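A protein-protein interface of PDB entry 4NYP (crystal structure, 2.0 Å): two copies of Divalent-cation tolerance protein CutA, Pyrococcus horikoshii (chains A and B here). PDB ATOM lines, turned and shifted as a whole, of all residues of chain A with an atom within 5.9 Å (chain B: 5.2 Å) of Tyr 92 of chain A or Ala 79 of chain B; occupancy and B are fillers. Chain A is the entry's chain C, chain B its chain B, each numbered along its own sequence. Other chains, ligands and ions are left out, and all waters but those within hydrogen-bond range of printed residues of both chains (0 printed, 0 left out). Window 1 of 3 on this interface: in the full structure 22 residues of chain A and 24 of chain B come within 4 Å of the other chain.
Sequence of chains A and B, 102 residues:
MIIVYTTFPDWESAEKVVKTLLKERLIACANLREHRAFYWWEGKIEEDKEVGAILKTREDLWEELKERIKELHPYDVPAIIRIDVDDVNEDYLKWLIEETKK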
ATOM      1  N   MET A   1       1.363 -17.060   1.149  1.00  0.00           N
ATOM      2  CA  MET A   1       2.054 -15.812   1.592  1.00  0.00           C
ATOM      3  C   MET A   1       2.709 -16.042   2.937  1.00  0.00           C
ATOM      4  O   MET A   1       2.468 -17.054   3.603  1.00  0.00           O
ATOM      5  CB  MET A   1       1.059 -14.652   1.727  1.00  0.00           C
ATOM      6  CG  MET A   1       0.019 -14.842   2.821  1.00  0.00           C
ATOM      7  SD  MET A   1      -1.068 -13.424   3.044  1.00  0.00           S
ATOM      8  CE  MET A   1      -0.018 -12.312   3.944  1.00  0.00           C
ATOM      9  N   CSD A  29       2.591  -4.819   2.271  1.00  0.00           N
ATOM     10  CA  CSD A  29       2.103  -4.040   3.398  1.00  0.00           C
ATOM     11  CB  CSD A  29       0.612  -4.333   3.562  1.00  0.00           C
ATOM     12  SG  CSD A  29      -0.034  -4.246   5.230  1.00  0.00           S
ATOM     13  C   CSD A  29       2.838  -4.310   4.710  1.00  0.00           C
ATOM     14  O   CSD A  29       3.438  -5.370   4.891  1.00  0.00           O
ATOM     15  OD1 CSD A  29      -0.448  -2.865   5.461  1.00  0.00           O
ATOM     16  OD2 CSD A  29      -1.118  -5.220   5.328  1.00  0.00           O
ATOM     17  N   LYS A  56       4.033  -8.220   5.226  1.00  0.00           N
ATOM     18  CA  LYS A  56       3.289  -9.216   4.467  1.00  0.00           C
ATOM     19  C   LYS A  56       3.800  -9.304   3.038  1.00  0.00           C
ATOM     20  O   LYS A  56       3.860  -8.297   2.318  1.00  0.00           O
ATOM     21  CB  LYS A  56       1.807  -8.854   4.496  1.00  0.00           C
ATOM     22  CG  LYS A  56       1.334  -8.562   5.918  1.00  0.00           C
ATOM     23  CD  LYS A  56      -0.001  -7.843   5.964  1.00  0.00           C
ATOM     24  CE  LYS A  56      -0.224  -7.250   7.348  1.00  0.00           C
ATOM     25  NZ  LYS A  56      -1.570  -6.633   7.495  1.00  0.00           N
ATOM     26  N   VAL A  88      -5.697 -17.745   3.978  1.00  0.00           N
ATOM     27  CA  VAL A  88      -6.107 -16.344   3.997  1.00  0.00           C
ATOM     28  C   VAL A  88      -7.177 -16.126   2.925  1.00  0.00           C
ATOM     29  O   VAL A  88      -7.274 -16.913   1.972  1.00  0.00           O
ATOM     30  CB  VAL A  88      -4.871 -15.425   3.737  1.00  0.00           C
ATOM     31  CG1 VAL A  88      -4.178 -15.848   2.454  1.00  0.00           C
ATOM     32  CG2 VAL A  88      -5.287 -13.961   3.663  1.00  0.00           C
ATOM     33  N   ASN A  89      -8.003 -15.092   3.084  1.00  0.00           N
ATOM     34  CA  ASN A  89      -9.024 -14.843   2.074  1.00  0.00           C
ATOM     35  C   ASN A  89      -8.271 -14.577   0.773  1.00  0.00           C
ATOM     36  O   ASN A  89      -7.324 -13.786   0.729  1.00  0.00           O
ATOM     37  CB  ASN A  89      -9.948 -13.681   2.471  1.00  0.00           C
ATOM     38  CG  ASN A  89      -9.202 -12.413   2.825  1.00  0.00           C
ATOM     39  OD1 ASN A  89      -8.237 -12.436   3.586  1.00  0.00           O
ATOM     40  ND2 ASN A  89      -9.668 -11.287   2.293  1.00  0.00           N
ATOM     41  N   GLU A  90      -8.690 -15.272  -0.279  1.00  0.00           N
ATOM     42  CA  GLU A  90      -8.030 -15.204  -1.570  1.00  0.00           C
ATOM     43  C   GLU A  90      -8.138 -13.920  -2.383  1.00  0.00           C
ATOM     44  O   GLU A  90      -7.413 -13.752  -3.364  1.00  0.00           O
ATOM     45  CB  GLU A  90      -8.452 -16.425  -2.384  1.00  0.00           C
ATOM     46  CG  GLU A  90      -8.323 -17.685  -1.535  1.00  0.00           C
ATOM     47  CD  GLU A  90      -8.536 -18.965  -2.295  1.00  0.00           C
ATOM     48  OE1 GLU A  90      -9.483 -19.027  -3.100  1.00  0.00           O
ATOM     49  OE2 GLU A  90      -7.756 -19.917  -2.067  1.00  0.00           O
ATOM     50  N   ASP A  91      -9.026 -13.012  -1.992  1.00  0.00           N
ATOM     51  CA  ASP A  91      -9.112 -11.749  -2.710  1.00  0.00           C
ATOM     52  C   ASP A  91      -7.971 -10.881  -2.175  1.00  0.00           C
ATOM     53  O   ASP A  91      -7.394 -10.072  -2.899  1.00  0.00           O
ATOM     54  CB  ASP A  91     -10.482 -11.081  -2.516  1.00  0.00           C
ATOM     55  CG  ASP A  91     -10.916 -11.010  -1.062  1.00  0.00           C
ATOM     56  OD1 ASP A  91     -10.750 -12.001  -0.318  1.00  0.00           O
ATOM     57  OD2 ASP A  91     -11.448  -9.953  -0.665  1.00  0.00           O
ATOM     58  N   TYR A  92      -7.631 -11.079  -0.904  1.00  0.00           N
ATOM     59  CA  TYR A  92      -6.532 -10.339  -0.295  1.00  0.00           C
ATOM     60  C   TYR A  92      -5.203 -10.871  -0.847  1.00  0.00           C
ATOM     61  O   TYR A  92      -4.304 -10.095  -1.168  1.00  0.00           O
ATOM     62  CB  TYR A  92      -6.568 -10.482   1.231  1.00  0.00           C
ATOM     63  CG  TYR A  92      -5.384  -9.845   1.935  1.00  0.00           C
ATOM     64  CD1 TYR A  92      -4.152 -10.494   1.994  1.00  0.00           C
ATOM     65  CD2 TYR A  92      -5.492  -8.583   2.525  1.00  0.00           C
ATOM     66  CE1 TYR A  92      -3.054  -9.908   2.619  1.00  0.00           C
ATOM     67  CE2 TYR A  92      -4.398  -7.984   3.156  1.00  0.00           C
ATOM     68  CZ  TYR A  92      -3.183  -8.655   3.197  1.00  0.00           C
ATOM     69  OH  TYR A  92      -2.094  -8.081   3.805  1.00  0.00           O
ATOM     70  N   LEU A  93      -5.090 -12.192  -0.973  1.00  0.00           N
ATOM     71  CA  LEU A  93      -3.868 -12.806  -1.493  1.00  0.00           C
ATOM     72  C   LEU A  93      -3.597 -12.395  -2.946  1.00  0.00           C
ATOM     73  O   LEU A  93      -2.439 -12.237  -3.353  1.00  0.00           O
ATOM     74  CB  LEU A  93      -3.959 -14.331  -1.389  1.00  0.00           C
ATOM     75  CG  LEU A  93      -2.715 -15.127  -1.797  1.00  0.00           C
ATOM     76  CD1 LEU A  93      -1.486 -14.595  -1.083  1.00  0.00           C
ATOM     77  CD2 LEU A  93      -2.926 -16.588  -1.462  1.00  0.00           C
ATOM     78  N   LYS A  94      -4.667 -12.237  -3.724  1.00  0.00           N
ATOM     79  CA  LYS A  94      -4.548 -11.820  -5.120  1.00  0.00           C
ATOM     80  C   LYS A  94      -3.935 -10.431  -5.104  1.00  0.00           C
ATOM     81  O   LYS A  94      -3.002 -10.138  -5.837  1.00  0.00           O
ATOM     82  CB  LYS A  94      -5.934 -11.759  -5.783  1.00  0.00           C
ATOM     83  CG  LYS A  94      -5.922 -11.217  -7.218  1.00  0.00           C
ATOM     84  CD  LYS A  94      -5.063 -12.102  -8.129  1.00  0.00           C
ATOM     85  CE  LYS A  94      -5.090 -11.625  -9.566  1.00  0.00           C
ATOM     86  NZ  LYS A  94      -4.293 -12.522 -10.444  1.00  0.00           N
ATOM     87  N   TRP A  95      -4.491  -9.574  -4.259  1.00  0.00           N
ATOM     88  CA  TRP A  95      -4.006  -8.213  -4.112  1.00  0.00           C
ATOM     89  C   TRP A  95      -2.521  -8.218  -3.726  1.00  0.00           C
ATOM     90  O   TRP A  95      -1.709  -7.515  -4.332  1.00  0.00           O
ATOM     91  CB  TRP A  95      -4.826  -7.487  -3.038  1.00  0.00           C
ATOM     92  CG  TRP A  95      -4.193  -6.211  -2.564  1.00  0.00           C
ATOM     93  CD1 TRP A  95      -4.226  -4.990  -3.186  1.00  0.00           C
ATOM     94  CD2 TRP A  95      -3.376  -6.044  -1.394  1.00  0.00           C
ATOM     95  NE1 TRP A  95      -3.478  -4.077  -2.475  1.00  0.00           N
ATOM     96  CE2 TRP A  95      -2.946  -4.698  -1.373  1.00  0.00           C
ATOM     97  CE3 TRP A  95      -2.966  -6.902  -0.366  1.00  0.00           C
ATOM     98  CZ2 TRP A  95      -2.123  -4.189  -0.358  1.00  0.00           C
ATOM     99  CZ3 TRP A  95      -2.143  -6.393   0.649  1.00  0.00           C
ATOM    100  CH2 TRP A  95      -1.734  -5.049   0.639  1.00  0.00           C
ATOM    101  N   LEU A  96      -2.170  -9.017  -2.723  1.00  0.00           N
ATOM    102  CA  LEU A  96      -0.788  -9.092  -2.264  1.00  0.00           C
ATOM    103  C   LEU A  96       0.171  -9.521  -3.377  1.00  0.00           C
ATOM    104  O   LEU A  96       1.225  -8.912  -3.569  1.00  0.00           O
ATOM    105  CB  LEU A  96      -0.681 -10.045  -1.062  1.00  0.00           C
ATOM    106  CG  LEU A  96       0.706 -10.148  -0.412  1.00  0.00           C
ATOM    107  CD1 LEU A  96       0.559 -10.384   1.092  1.00  0.00           C
ATOM    108  CD2 LEU A  96       1.502 -11.271  -1.062  1.00  0.00           C
ATOM    109  N   ILE A  97      -0.192 -10.562  -4.117  1.00  0.00           N
ATOM    110  CA  ILE A  97       0.653 -11.031  -5.205  1.00  0.00           C
ATOM    111  C   ILE A  97       0.817  -9.955  -6.287  1.00  0.00           C
ATOM    112  O   ILE A  97       1.916  -9.740  -6.790  1.00  0.00           O
ATOM    113  CB  ILE A  97       0.075 -12.309  -5.848  1.00  0.00           C
ATOM    114  CG1 ILE A  97       0.135 -13.464  -4.847  1.00  0.00           C
ATOM    115  CG2 ILE A  97       0.862 -12.669  -7.098  1.00  0.00           C
ATOM    116  CD1 ILE A  97      -0.563 -14.732  -5.331  1.00  0.00           C
ATOM    117  N   TYR B   5      -5.749 -13.206  12.053  1.00  0.00           N
ATOM    118  CA  TYR B   5      -5.383 -11.802  12.139  1.00  0.00           C
ATOM    119  C   TYR B   5      -6.104 -10.988  11.072  1.00  0.00           C
ATOM    120  O   TYR B   5      -6.100 -11.348   9.895  1.00  0.00           O
ATOM    121  CB  TYR B   5      -3.871 -11.648  11.968  1.00  0.00           C
ATOM    122  CG  TYR B   5      -3.353 -10.226  12.090  1.00  0.00           C
ATOM    123  CD1 TYR B   5      -2.630  -9.638  11.051  1.00  0.00           C
ATOM    124  CD2 TYR B   5      -3.552  -9.485  13.257  1.00  0.00           C
ATOM    125  CE1 TYR B   5      -2.115  -8.347  11.172  1.00  0.00           C
ATOM    126  CE2 TYR B   5      -3.039  -8.193  13.391  1.00  0.00           C
ATOM    127  CZ  TYR B   5      -2.320  -7.632  12.344  1.00  0.00           C
ATOM    128  OH  TYR B   5      -1.788  -6.367  12.475  1.00  0.00           O
ATOM    129  N   THR B   6      -6.739  -9.903  11.502  1.00  0.00           N
ATOM    130  CA  THR B   6      -7.440  -9.010  10.597  1.00  0.00           C
ATOM    131  C   THR B   6      -7.238  -7.586  11.115  1.00  0.00           C
ATOM    132  O   THR B   6      -6.821  -7.390  12.263  1.00  0.00           O
ATOM    133  CB  THR B   6      -8.950  -9.339  10.531  1.00  0.00           C
ATOM    134  OG1 THR B   6      -9.556  -8.583   9.473  1.00  0.00           O
ATOM    135  CG2 THR B   6      -9.632  -9.004  11.849  1.00  0.00           C
ATOM    136  N   THR B   7      -7.508  -6.590  10.275  1.00  0.00           N
ATOM    137  CA  THR B   7      -7.336  -5.205  10.703  1.00  0.00           C
ATOM    138  C   THR B   7      -8.597  -4.408  10.406  1.00  0.00           C
ATOM    139  O   THR B   7      -9.352  -4.756   9.506  1.00  0.00           O
ATOM    140  CB  THR B   7      -6.130  -4.539   9.999  1.00  0.00           C
ATOM    141  OG1 THR B   7      -6.452  -4.268   8.630  1.00  0.00           O
ATOM    142  CG2 THR B   7      -4.921  -5.461  10.042  1.00  0.00           C
ATOM    143  N   VAL B  77     -11.634  -5.299   0.711  1.00  0.00           N
ATOM    144  CA  VAL B  77     -10.669  -6.392   0.623  1.00  0.00           C
ATOM    145  C   VAL B  77      -9.871  -6.421   1.927  1.00  0.00           C
ATOM    146  O   VAL B  77      -8.722  -5.986   1.979  1.00  0.00           O
ATOM    147  CB  VAL B  77      -9.697  -6.204  -0.564  1.00  0.00           C
ATOM    148  CG1 VAL B  77      -8.846  -7.460  -0.744  1.00  0.00           C
ATOM    149  CG2 VAL B  77     -10.472  -5.905  -1.831  1.00  0.00           C
ATOM    150  N   PRO B  78     -10.484  -6.935   3.005  1.00  0.00           N
ATOM    151  CA  PRO B  78      -9.819  -7.011   4.308  1.00  0.00           C
ATOM    152  C   PRO B  78      -8.785  -8.125   4.396  1.00  0.00           C
ATOM    153  O   PRO B  78      -8.754  -9.029   3.570  1.00  0.00           O
ATOM    154  CB  PRO B  78     -10.979  -7.248   5.261  1.00  0.00           C
ATOM    155  CG  PRO B  78     -11.873  -8.146   4.444  1.00  0.00           C
ATOM    156  CD  PRO B  78     -11.857  -7.467   3.086  1.00  0.00           C
ATOM    157  N   ALA B  79      -7.931  -8.041   5.408  1.00  0.00           N
ATOM    158  CA  ALA B  79      -6.924  -9.063   5.633  1.00  0.00           C
ATOM    159  C   ALA B  79      -7.522 -10.054   6.627  1.00  0.00           C
ATOM    160  O   ALA B  79      -7.911  -9.668   7.727  1.00  0.00           O
ATOM    161  CB  ALA B  79      -5.659  -8.439   6.217  1.00  0.00           C
ATOM    162  N   ILE B  80      -7.631 -11.316   6.226  1.00  0.00           N
ATOM    163  CA  ILE B  80      -8.151 -12.354   7.116  1.00  0.00           C
ATOM    164  C   ILE B  80      -7.104 -13.455   7.035  1.00  0.00           C
ATOM    165  O   ILE B  80      -7.227 -14.396   6.251  1.00  0.00           O
ATOM    166  CB  ILE B  80      -9.507 -12.892   6.639  1.00  0.00           C
ATOM    167  CG1 ILE B  80     -10.446 -11.728   6.310  1.00  0.00           C
ATOM    168  CG2 ILE B  80     -10.123 -13.764   7.726  1.00  0.00           C
ATOM    169  CD1 ILE B  80     -11.790 -12.160   5.754  1.00  0.00           C
ATOM    170  N   ILE B  81      -6.073 -13.316   7.866  1.00  0.00           N
ATOM    171  CA  ILE B  81      -4.927 -14.219   7.887  1.00  0.00           C
ATOM    172  C   ILE B  81      -4.978 -15.317   8.944  1.00  0.00           C
ATOM    173  O   ILE B  81      -5.100 -15.037  10.136  1.00  0.00           O
ATOM    174  CB  ILE B  81      -3.632 -13.380   8.073  1.00  0.00           C
ATOM    175  CG1 ILE B  81      -3.472 -12.428   6.880  1.00  0.00           C
ATOM    176  CG2 ILE B  81      -2.412 -14.286   8.216  1.00  0.00           C
ATOM    177  CD1 ILE B  81      -2.424 -11.350   7.082  1.00  0.00           C
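Of the 13 printed residues of chain A, 4 touch a printed residue of chain B.
Printed residues of chain A that touch a printed residue of chain B: Val 88, Asn 89, Asp 91 and Tyr 92.
Hydrophobic or aromatic side chains of chain A that line the printed part of chain B: Val 88 and Tyr 92.
Of the 8 printed residues of chain B, 5 touch a printed residue of chain A.
Printed residues of chain B that touch a printed residue of chain A: Val 77, Pro 78, Ala 79, Ile 80 and Ile 81.
Hydrophobic or aromatic side chains of chain B that line the printed part of chain A: Val 77, Ala 79, Ile 80 and Ile 81.
Among the printed residues, no Asp or Glu carboxylate lies within 4 Å of a Lys or Arg side-chain nitrogen of the other chain.
Of the printed residues of chain B, Val 88 of chain A touches Ile 80 (3.2 Å) and Ile 81 (3.999 Å).
Printed residues of chain B within 4 Å of Asn 89 of chain A: Pro 78, Ala 79 and Ile 80.
Of chain B, only Val 77, Pro 78 and Ala 79 come within 4 Å of Tyr 92 of chain A.
Ile 97 of chain A touches none of the printed residues of chain B.
Of the printed residues of chain A, Val 77 of chain B touches Asp 91 (3.6 Å) and Tyr 92 (3.7 Å).
Of the printed residues of chain A, Pro 78 of chain B touches Asn 89 (2.8 Å) and Tyr 92 (3.5 Å).
Of chain A, only Asn 89 and Tyr 92 come within 4 Å of Ala 79 of chain B.
Printed residues of chain A within 4 Å of Ile 81 of chain B: Val 88 (3.999 Å).
The nearest residue of chain B that does not touch Tyr 92 of chain A is Ile 81 of chain B (4.6 Å).
The nearest residue of chain A that does not touch Ala 79 of chain B is Lys 56 of chain A (4.6 Å).
The nearest printed residue of chain A that does not touch Ile 80 of chain B is Tyr 92 of chain A (5.1 Å).
Among the printed residues, merely in contact across the chains: Val 88 of chain A with Ile 80 of chain B, Val 88 of chain A with Ile 81 of chain B, Asn 89 of chain A with Ala 79 of chain B, Asp 91 of chain A with Val 77 of chain B, Tyr 92 of chain A with Val 77 of chain B, Tyr 92 of chain A with Pro 78 of chain B and Tyr 92 of chain A with Ala 79 of chain B.
The backbone carbonyl oxygen (O) of Ile 81 of chain B sits at hydrogen-bond distance from the backbone NH (N) of Tyr 5 of chain B, 2.7 Å away.
OG1 of Thr 6 of chain B is in hydrogen-bond range of O of Ala 79 of chain B (2.6 Å).
OD2 of CSD 29 of chain A lies within hydrogen-bond range of the side-chain hydroxyl of Tyr 92 of chain A, at 3.4 Å.
The side-chain carboxylate (OD1) of Asp 91 of chain A is in hydrogen-bond range of the side-chain amide nitrogen (ND2) of Asn 89 of chain A (2.9 Å).
ND2 of Asn 89 of chain A is in hydrogen-bond range of O of Pro 78 of chain B (2.8 Å).
The side-chain amide oxygen (OD1) of Asn 89 of chain A lies within hydrogen-bond range of the backbone NH (N) of Ile 80 of chain B, 2.9 Å away.
No position is printed for both chains.
Of the 9 pairs that touch across the chains among the printed residues, none has its exchanged pair printed and touching as well.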
